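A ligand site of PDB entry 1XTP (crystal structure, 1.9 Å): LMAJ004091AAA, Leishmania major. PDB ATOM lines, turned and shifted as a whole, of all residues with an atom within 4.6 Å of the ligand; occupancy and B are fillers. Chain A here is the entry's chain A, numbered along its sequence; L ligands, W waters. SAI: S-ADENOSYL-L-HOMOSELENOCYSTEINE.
Trp 57 touches the ligand (CH2 to SE, 3.4 Å).
Val 67 touches the ligand (O to SE, 3.6 Å).
Ala 102 touches the ligand.
Gly 103 touches the ligand.
Ile 107 touches the ligand (CD1 to O, 3.4 Å).
Pro 124 touches the ligand (CD to N3, 3.2 Å).
Val 125 touches the ligand (CG2 to O2', 3.2 Å).
Ser 148 touches the ligand.
Trp 166 touches the ligand.
Tyr 170 touches the ligand.
OE2 of Glu 123 is in hydrogen-bond range of N of Val 125, at 2.9 Å.
The side-chain carboxylate (OE1) of Glu 123 lies within hydrogen-bond range of the backbone NH (N) of Gly 103 (2.7 Å).
The side-chain carboxylate of Glu 123 is in hydrogen-bond range of the backbone NH of Ala 102.
The backbone NH (N) of Ala 147 sits at hydrogen-bond distance from the backbone carbonyl oxygen (O) of Glu 123 (3.2 Å).
The backbone NH of Gly 101 sits at hydrogen-bond distance from the backbone carbonyl oxygen of Leu 122.
NE1 of Trp 57 sits at hydrogen-bond distance from OH of Tyr 170 (2.8 Å).
N of Ala 102 is in hydrogen-bond range of O of Leu 122.
Water W1 lies within hydrogen-bond range of O of Ala 102 (2.6 Å), OXT of the ligand (2.7 Å) and N of Arg 106 (3.2 Å).
Water W3 bridges the backbone carbonyl oxygen (O) of Cys 100 (2.5 Å) and a nitrogen (N) of the ligand (2.9 Å).
Water W4 lies within hydrogen-bond range of OG of Ser 148, OE2 of Glu 150 and N6 of the ligand.
OE2 of Glu 123 lies within hydrogen-bond range of O2' of the ligand, 2.6 Å away.
O of Gly 101 lies within hydrogen-bond range of N of the ligand, 2.8 Å away.
An oxygen (OXT) of the ligand is in salt-bridge range of the guanidinium group (NE) of Arg 106, 2.8 Å away.
N of Met 149 is in hydrogen-bond range of N1 of the ligand, at 3.0 Å.
O of Gln 165 lies within hydrogen-bond range of N of the ligand, at 3.0 Å.
N6 of the ligand is in hydrogen-bond range of OE1 of Glu 150.
The side-chain hydroxyl (OG1) of Thr 167 lies within hydrogen-bond range of an oxygen (O4') of the ligand (3.1 Å).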
ATOM      1  N   TYR A  50       0.687   3.259 -13.441  1.00  0.00           N
ATOM      2  CA  TYR A  50       1.525   2.255 -14.078  1.00  0.00           C
ATOM      3  C   TYR A  50       2.379   1.500 -13.081  1.00  0.00           C
ATOM      4  O   TYR A  50       2.479   0.276 -13.168  1.00  0.00           O
ATOM      5  CB  TYR A  50       2.424   2.876 -15.155  1.00  0.00           C
ATOM      6  CG  TYR A  50       1.695   3.287 -16.382  1.00  0.00           C
ATOM      7  CD1 TYR A  50       1.085   2.333 -17.211  1.00  0.00           C
ATOM      8  CD2 TYR A  50       1.612   4.626 -16.755  1.00  0.00           C
ATOM      9  CE1 TYR A  50       0.403   2.719 -18.339  1.00  0.00           C
ATOM     10  CE2 TYR A  50       0.944   5.017 -17.889  1.00  0.00           C
ATOM     11  CZ  TYR A  50       0.330   4.044 -18.681  1.00  0.00           C
ATOM     12  OH  TYR A  50      -0.338   4.427 -19.807  1.00  0.00           O
ATOM     13  N   LEU A  54       2.954  -2.713 -12.448  1.00  0.00           N
ATOM     14  CA  LEU A  54       4.265  -3.329 -12.597  1.00  0.00           C
ATOM     15  C   LEU A  54       4.709  -3.968 -11.302  1.00  0.00           C
ATOM     16  O   LEU A  54       5.330  -5.007 -11.306  1.00  0.00           O
ATOM     17  CB  LEU A  54       5.297  -2.288 -13.047  1.00  0.00           C
ATOM     18  CG  LEU A  54       5.114  -1.676 -14.433  1.00  0.00           C
ATOM     19  CD1 LEU A  54       6.254  -0.714 -14.738  1.00  0.00           C
ATOM     20  CD2 LEU A  54       4.977  -2.745 -15.517  1.00  0.00           C
ATOM     21  N   TRP A  57       2.782  -7.176 -10.874  1.00  0.00           N
ATOM     22  CA  TRP A  57       3.256  -8.267 -11.707  1.00  0.00           C
ATOM     23  C   TRP A  57       4.616  -8.794 -11.301  1.00  0.00           C
ATOM     24  O   TRP A  57       4.933  -9.913 -11.657  1.00  0.00           O
ATOM     25  CB  TRP A  57       3.231  -7.890 -13.173  1.00  0.00           C
ATOM     26  CG  TRP A  57       1.849  -8.041 -13.707  1.00  0.00           C
ATOM     27  CD1 TRP A  57       0.923  -7.047 -13.843  1.00  0.00           C
ATOM     28  CD2 TRP A  57       1.214  -9.245 -14.132  1.00  0.00           C
ATOM     29  NE1 TRP A  57      -0.224  -7.554 -14.348  1.00  0.00           N
ATOM     30  CE2 TRP A  57      -0.087  -8.908 -14.519  1.00  0.00           C
ATOM     31  CE3 TRP A  57       1.635 -10.580 -14.223  1.00  0.00           C
ATOM     32  CZ2 TRP A  57      -0.987  -9.848 -15.030  1.00  0.00           C
ATOM     33  CZ3 TRP A  57       0.720 -11.525 -14.729  1.00  0.00           C
ATOM     34  CH2 TRP A  57      -0.563 -11.156 -15.108  1.00  0.00           C
ATOM     35  N   VAL A  67      -0.228 -15.861 -15.826  1.00  0.00           N
ATOM     36  CA  VAL A  67      -0.681 -14.900 -16.831  1.00  0.00           C
ATOM     37  C   VAL A  67      -2.177 -15.005 -17.049  1.00  0.00           C
ATOM     38  O   VAL A  67      -2.795 -14.048 -17.494  1.00  0.00           O
ATOM     39  CB  VAL A  67       0.116 -14.983 -18.181  1.00  0.00           C
ATOM     40  CG1 VAL A  67       1.584 -14.707 -17.937  1.00  0.00           C
ATOM     41  CG2 VAL A  67      -0.077 -16.291 -18.899  1.00  0.00           C
ATOM     42  N   CYS A 100       2.724  -8.034 -27.717  1.00  0.00           N
ATOM     43  CA  CYS A 100       2.797  -6.920 -26.759  1.00  0.00           C
ATOM     44  C   CYS A 100       2.210  -7.332 -25.414  1.00  0.00           C
ATOM     45  O   CYS A 100       1.152  -7.963 -25.359  1.00  0.00           O
ATOM     46  CB  CYS A 100       1.978  -5.726 -27.248  1.00  0.00           C
ATOM     47  SG  CYS A 100       2.500  -4.982 -28.757  1.00  0.00           S
ATOM     48  N   GLY A 101       2.862  -6.927 -24.331  1.00  0.00           N
ATOM     49  CA  GLY A 101       2.500  -7.429 -23.003  1.00  0.00           C
ATOM     50  C   GLY A 101       2.532  -8.954 -23.024  1.00  0.00           C
ATOM     51  O   GLY A 101       1.605  -9.598 -22.576  1.00  0.00           O
ATOM     52  N   ALA A 102       3.627  -9.496 -23.550  1.00  0.00           N
ATOM     53  CA  ALA A 102       3.770 -10.925 -23.856  1.00  0.00           C
ATOM     54  C   ALA A 102       3.785 -11.859 -22.652  1.00  0.00           C
ATOM     55  O   ALA A 102       3.465 -13.036 -22.793  1.00  0.00           O
ATOM     56  CB  ALA A 102       5.021 -11.141 -24.652  1.00  0.00           C
ATOM     57  N   GLY A 103       4.170 -11.331 -21.481  1.00  0.00           N
ATOM     58  CA  GLY A 103       4.303 -12.135 -20.291  1.00  0.00           C
ATOM     59  C   GLY A 103       5.357 -13.188 -20.497  1.00  0.00           C
ATOM     60  O   GLY A 103       6.501 -12.872 -20.805  1.00  0.00           O
ATOM     61  N   ARG A 106       3.181 -16.891 -23.951  1.00  0.00           N
ATOM     62  CA  ARG A 106       2.128 -17.886 -24.186  1.00  0.00           C
ATOM     63  C   ARG A 106       1.502 -17.829 -25.571  1.00  0.00           C
ATOM     64  O   ARG A 106       1.297 -18.886 -26.234  1.00  0.00           O
ATOM     65  CB  ARG A 106       1.018 -17.715 -23.131  1.00  0.00           C
ATOM     66  CG  ARG A 106      -0.128 -18.748 -23.236  1.00  0.00           C
ATOM     67  CD  ARG A 106      -1.283 -18.381 -22.278  1.00  0.00           C
ATOM     68  NE  ARG A 106      -1.941 -17.144 -22.702  1.00  0.00           N
ATOM     69  CZ  ARG A 106      -2.933 -17.062 -23.569  1.00  0.00           C
ATOM     70  NH1 ARG A 106      -3.485 -18.139 -24.121  1.00  0.00           N
ATOM     71  NH2 ARG A 106      -3.419 -15.869 -23.886  1.00  0.00           N
ATOM     72  N   ILE A 107       1.148 -16.619 -26.019  1.00  0.00           N
ATOM     73  CA  ILE A 107       0.560 -16.455 -27.314  1.00  0.00           C
ATOM     74  C   ILE A 107       1.589 -16.724 -28.444  1.00  0.00           C
ATOM     75  O   ILE A 107       1.276 -17.382 -29.458  1.00  0.00           O
ATOM     76  CB  ILE A 107      -0.114 -15.049 -27.477  1.00  0.00           C
ATOM     77  CG1 ILE A 107      -1.246 -14.890 -26.440  1.00  0.00           C
ATOM     78  CG2 ILE A 107      -0.670 -14.872 -28.913  1.00  0.00           C
ATOM     79  CD1 ILE A 107      -1.787 -13.473 -26.302  1.00  0.00           C
ATOM     80  N   LEU A 122       7.333  -8.034 -26.520  1.00  0.00           N
ATOM     81  CA  LEU A 122       7.431  -6.793 -25.790  1.00  0.00           C
ATOM     82  C   LEU A 122       6.824  -7.021 -24.403  1.00  0.00           C
ATOM     83  O   LEU A 122       5.647  -7.317 -24.316  1.00  0.00           O
ATOM     84  CB  LEU A 122       6.697  -5.680 -26.549  1.00  0.00           C
ATOM     85  CG  LEU A 122       6.659  -4.269 -25.904  1.00  0.00           C
ATOM     86  CD1 LEU A 122       6.451  -3.217 -26.953  1.00  0.00           C
ATOM     87  CD2 LEU A 122       5.578  -4.147 -24.835  1.00  0.00           C
ATOM     88  N   GLU A 123       7.594  -6.858 -23.342  1.00  0.00           N
ATOM     89  CA  GLU A 123       7.135  -7.173 -22.000  1.00  0.00           C
ATOM     90  C   GLU A 123       7.993  -6.383 -21.042  1.00  0.00           C
ATOM     91  O   GLU A 123       9.212  -6.425 -21.181  1.00  0.00           O
ATOM     92  CB  GLU A 123       7.297  -8.669 -21.746  1.00  0.00           C
ATOM     93  CG  GLU A 123       7.134  -9.125 -20.299  1.00  0.00           C
ATOM     94  CD  GLU A 123       5.809  -8.698 -19.678  1.00  0.00           C
ATOM     95  OE1 GLU A 123       4.767  -8.923 -20.321  1.00  0.00           O
ATOM     96  OE2 GLU A 123       5.811  -8.117 -18.562  1.00  0.00           O
ATOM     97  N   PRO A 124       7.390  -5.615 -20.119  1.00  0.00           N
ATOM     98  CA  PRO A 124       8.154  -4.780 -19.177  1.00  0.00           C
ATOM     99  C   PRO A 124       8.665  -5.470 -17.936  1.00  0.00           C
ATOM    100  O   PRO A 124       9.569  -4.944 -17.286  1.00  0.00           O
ATOM    101  CB  PRO A 124       7.123  -3.723 -18.772  1.00  0.00           C
ATOM    102  CG  PRO A 124       5.829  -4.458 -18.817  1.00  0.00           C
ATOM    103  CD  PRO A 124       5.935  -5.368 -19.991  1.00  0.00           C
ATOM    104  N   VAL A 125       8.077  -6.602 -17.575  1.00  0.00           N
ATOM    105  CA  VAL A 125       8.480  -7.299 -16.349  1.00  0.00           C
ATOM    106  C   VAL A 125       9.558  -8.314 -16.612  1.00  0.00           C
ATOM    107  O   VAL A 125       9.380  -9.267 -17.365  1.00  0.00           O
ATOM    108  CB  VAL A 125       7.291  -7.958 -15.635  1.00  0.00           C
ATOM    109  CG1 VAL A 125       7.749  -8.667 -14.381  1.00  0.00           C
ATOM    110  CG2 VAL A 125       6.262  -6.872 -15.287  1.00  0.00           C
ATOM    111  N   MET A 128       9.225 -12.102 -16.193  1.00  0.00           N
ATOM    112  CA  MET A 128       8.287 -12.623 -17.195  1.00  0.00           C
ATOM    113  C   MET A 128       9.028 -12.796 -18.534  1.00  0.00           C
ATOM    114  O   MET A 128       8.937 -13.842 -19.176  1.00  0.00           O
ATOM    115  CB  MET A 128       7.084 -11.690 -17.393  1.00  0.00           C
ATOM    116  CG  MET A 128       6.264 -11.410 -16.149  1.00  0.00           C
ATOM    117  SD  MET A 128       5.350 -13.004 -15.506  1.00  0.00           S
ATOM    118  CE  MET A 128       4.296 -13.321 -16.947  1.00  0.00           C
ATOM    119  N   ALA A 147      10.225  -3.521 -22.204  1.00  0.00           N
ATOM    120  CA  ALA A 147       9.634  -2.202 -22.165  1.00  0.00           C
ATOM    121  C   ALA A 147       8.137  -2.319 -21.943  1.00  0.00           C
ATOM    122  O   ALA A 147       7.543  -3.365 -22.209  1.00  0.00           O
ATOM    123  CB  ALA A 147       9.921  -1.457 -23.473  1.00  0.00           C
ATOM    124  N   SER A 148       7.536  -1.253 -21.410  1.00  0.00           N
ATOM    125  CA  SER A 148       6.084  -1.107 -21.430  1.00  0.00           C
ATOM    126  C   SER A 148       5.656  -0.598 -22.798  1.00  0.00           C
ATOM    127  O   SER A 148       6.457  -0.015 -23.541  1.00  0.00           O
ATOM    128  CB  SER A 148       5.640  -0.148 -20.348  1.00  0.00           C
ATOM    129  OG  SER A 148       6.102  -0.557 -19.057  1.00  0.00           O
ATOM    130  N   MET A 149       4.394  -0.822 -23.135  1.00  0.00           N
ATOM    131  CA  MET A 149       3.846  -0.416 -24.417  1.00  0.00           C
ATOM    132  C   MET A 149       3.973   1.090 -24.573  1.00  0.00           C
ATOM    133  O   MET A 149       4.366   1.568 -25.656  1.00  0.00           O
ATOM    134  CB  MET A 149       2.369  -0.807 -24.550  1.00  0.00           C
ATOM    135  CG  MET A 149       2.111  -2.287 -24.848  1.00  0.00           C
ATOM    136  SD  MET A 149       0.202  -2.724 -24.812  1.00  0.00           S
ATOM    137  CE  MET A 149      -0.131  -2.622 -22.849  1.00  0.00           C
ATOM    138  N   GLU A 150       3.668   1.809 -23.508  1.00  0.00           N
ATOM    139  CA  GLU A 150       3.595   3.269 -23.549  1.00  0.00           C
ATOM    140  C   GLU A 150       4.976   3.960 -23.605  1.00  0.00           C
ATOM    141  O   GLU A 150       5.043   5.182 -23.791  1.00  0.00           O
ATOM    142  CB  GLU A 150       2.746   3.817 -22.382  1.00  0.00           C
ATOM    143  CG  GLU A 150       3.399   3.859 -20.975  1.00  0.00           C
ATOM    144  CD  GLU A 150       3.385   2.502 -20.246  1.00  0.00           C
ATOM    145  OE1 GLU A 150       2.818   1.530 -20.780  1.00  0.00           O
ATOM    146  OE2 GLU A 150       3.960   2.418 -19.134  1.00  0.00           O
ATOM    147  N   GLN A 165      -3.206  -8.480 -26.240  1.00  0.00           N
ATOM    148  CA  GLN A 165      -4.186  -9.311 -25.574  1.00  0.00           C
ATOM    149  C   GLN A 165      -4.003  -9.257 -24.078  1.00  0.00           C
ATOM    150  O   GLN A 165      -2.910  -9.506 -23.585  1.00  0.00           O
ATOM    151  CB  GLN A 165      -4.082 -10.770 -26.023  1.00  0.00           C
ATOM    152  CG  GLN A 165      -4.967 -11.702 -25.179  1.00  0.00           C
ATOM    153  CD  GLN A 165      -5.332 -13.008 -25.887  1.00  0.00           C
ATOM    154  OE1 GLN A 165      -4.910 -13.266 -27.016  1.00  0.00           O
ATOM    155  NE2 GLN A 165      -6.136 -13.841 -25.201  1.00  0.00           N
ATOM    156  N   TRP A 166      -5.098  -8.939 -23.378  1.00  0.00           N
ATOM    157  CA  TRP A 166      -5.130  -8.907 -21.906  1.00  0.00           C
ATOM    158  C   TRP A 166      -4.045  -7.977 -21.309  1.00  0.00           C
ATOM    159  O   TRP A 166      -3.484  -8.236 -20.235  1.00  0.00           O
ATOM    160  CB  TRP A 166      -5.072 -10.330 -21.334  1.00  0.00           C
ATOM    161  CG  TRP A 166      -6.392 -11.079 -21.442  1.00  0.00           C
ATOM    162  CD1 TRP A 166      -7.650 -10.553 -21.318  1.00  0.00           C
ATOM    163  CD2 TRP A 166      -6.580 -12.480 -21.672  1.00  0.00           C
ATOM    164  NE1 TRP A 166      -8.605 -11.527 -21.482  1.00  0.00           N
ATOM    165  CE2 TRP A 166      -7.972 -12.727 -21.695  1.00  0.00           C
ATOM    166  CE3 TRP A 166      -5.708 -13.552 -21.877  1.00  0.00           C
ATOM    167  CZ2 TRP A 166      -8.507 -13.995 -21.902  1.00  0.00           C
ATOM    168  CZ3 TRP A 166      -6.243 -14.820 -22.084  1.00  0.00           C
ATOM    169  CH2 TRP A 166      -7.636 -15.020 -22.103  1.00  0.00           C
ATOM    170  N   THR A 167      -3.762  -6.886 -22.010  1.00  0.00           N
ATOM    171  CA  THR A 167      -2.698  -5.988 -21.596  1.00  0.00           C
ATOM    172  C   THR A 167      -3.075  -4.521 -21.780  1.00  0.00           C
ATOM    173  O   THR A 167      -2.625  -3.667 -21.030  1.00  0.00           O
ATOM    174  CB  THR A 167      -1.356  -6.384 -22.297  1.00  0.00           C
ATOM    175  OG1 THR A 167      -0.237  -5.800 -21.630  1.00  0.00           O
ATOM    176  CG2 THR A 167      -1.372  -6.008 -23.792  1.00  0.00           C
ATOM    177  N   TYR A 170      -3.991  -1.991 -18.839  1.00  0.00           N
ATOM    178  CA  TYR A 170      -2.994  -1.250 -18.048  1.00  0.00           C
ATOM    179  C   TYR A 170      -2.675   0.130 -18.586  1.00  0.00           C
ATOM    180  O   TYR A 170      -2.091   0.946 -17.877  1.00  0.00           O
ATOM    181  CB  TYR A 170      -1.709  -2.088 -17.937  1.00  0.00           C
ATOM    182  CG  TYR A 170      -1.970  -3.397 -17.255  1.00  0.00           C
ATOM    183  CD1 TYR A 170      -2.339  -3.431 -15.922  1.00  0.00           C
ATOM    184  CD2 TYR A 170      -1.914  -4.603 -17.960  1.00  0.00           C
ATOM    185  CE1 TYR A 170      -2.625  -4.627 -15.288  1.00  0.00           C
ATOM    186  CE2 TYR A 170      -2.175  -5.820 -17.327  1.00  0.00           C
ATOM    187  CZ  TYR A 170      -2.552  -5.811 -15.995  1.00  0.00           C
ATOM    188  OH  TYR A 170      -2.835  -6.978 -15.330  1.00  0.00           O
HETATM  189  N   SAI L   1      -0.487 -11.240 -23.308  1.00  0.00           N
HETATM  190  CA  SAI L   1      -0.035 -12.416 -22.528  1.00  0.00           C
HETATM  191  CB  SAI L   1       0.093 -12.058 -21.063  1.00  0.00           C
HETATM  192  CG  SAI L   1      -1.177 -11.611 -20.366  1.00  0.00           C
HETATM  193 SE   SAI L   1      -0.775 -11.195 -18.477  1.00  0.00          SE
HETATM  194  C   SAI L   1      -0.996 -13.592 -22.598  1.00  0.00           C
HETATM  195  O   SAI L   1      -2.166 -13.430 -22.964  1.00  0.00           O
HETATM  196  OXT SAI L   1      -0.644 -14.714 -22.262  1.00  0.00           O
HETATM  197  C5' SAI L   1      -0.545  -9.246 -18.719  1.00  0.00           C
HETATM  198  C4' SAI L   1       0.892  -8.842 -19.062  1.00  0.00           C
HETATM  199  O4' SAI L   1       0.914  -7.464 -19.314  1.00  0.00           O
HETATM  200  C3' SAI L   1       1.911  -9.081 -17.960  1.00  0.00           C
HETATM  201  O3' SAI L   1       3.009  -9.793 -18.443  1.00  0.00           O
HETATM  202  C2' SAI L   1       2.368  -7.705 -17.510  1.00  0.00           C
HETATM  203  O2' SAI L   1       3.718  -7.679 -17.099  1.00  0.00           O
HETATM  204  C1' SAI L   1       2.125  -6.952 -18.790  1.00  0.00           C
HETATM  205  N9  SAI L   1       1.995  -5.506 -18.638  1.00  0.00           N
HETATM  206  C8  SAI L   1       1.512  -4.823 -17.546  1.00  0.00           C
HETATM  207  N7  SAI L   1       1.560  -3.522 -17.815  1.00  0.00           N
HETATM  208  C5  SAI L   1       2.063  -3.371 -19.084  1.00  0.00           C
HETATM  209  C6  SAI L   1       2.314  -2.236 -19.863  1.00  0.00           C
HETATM  210  N6  SAI L   1       2.065  -1.028 -19.371  1.00  0.00           N
HETATM  211  N1  SAI L   1       2.837  -2.400 -21.136  1.00  0.00           N
HETATM  212  C2  SAI L   1       3.131  -3.654 -21.637  1.00  0.00           C
HETATM  213  N3  SAI L   1       2.869  -4.770 -20.855  1.00  0.00           N
HETATM  214  C4  SAI L   1       2.331  -4.616 -19.610  1.00  0.00           C
HETATM  215  O   HOH W   1       1.969 -14.903 -21.695  1.00  0.00           O
HETATM  216  O   HOH W   2       1.593  -1.018 -16.570  1.00  0.00           O
HETATM  217  O   HOH W   3      -0.041 -10.097 -25.891  1.00  0.00           O
HETATM  218  O   HOH W   4       4.016   0.230 -17.506  1.00  0.00           O
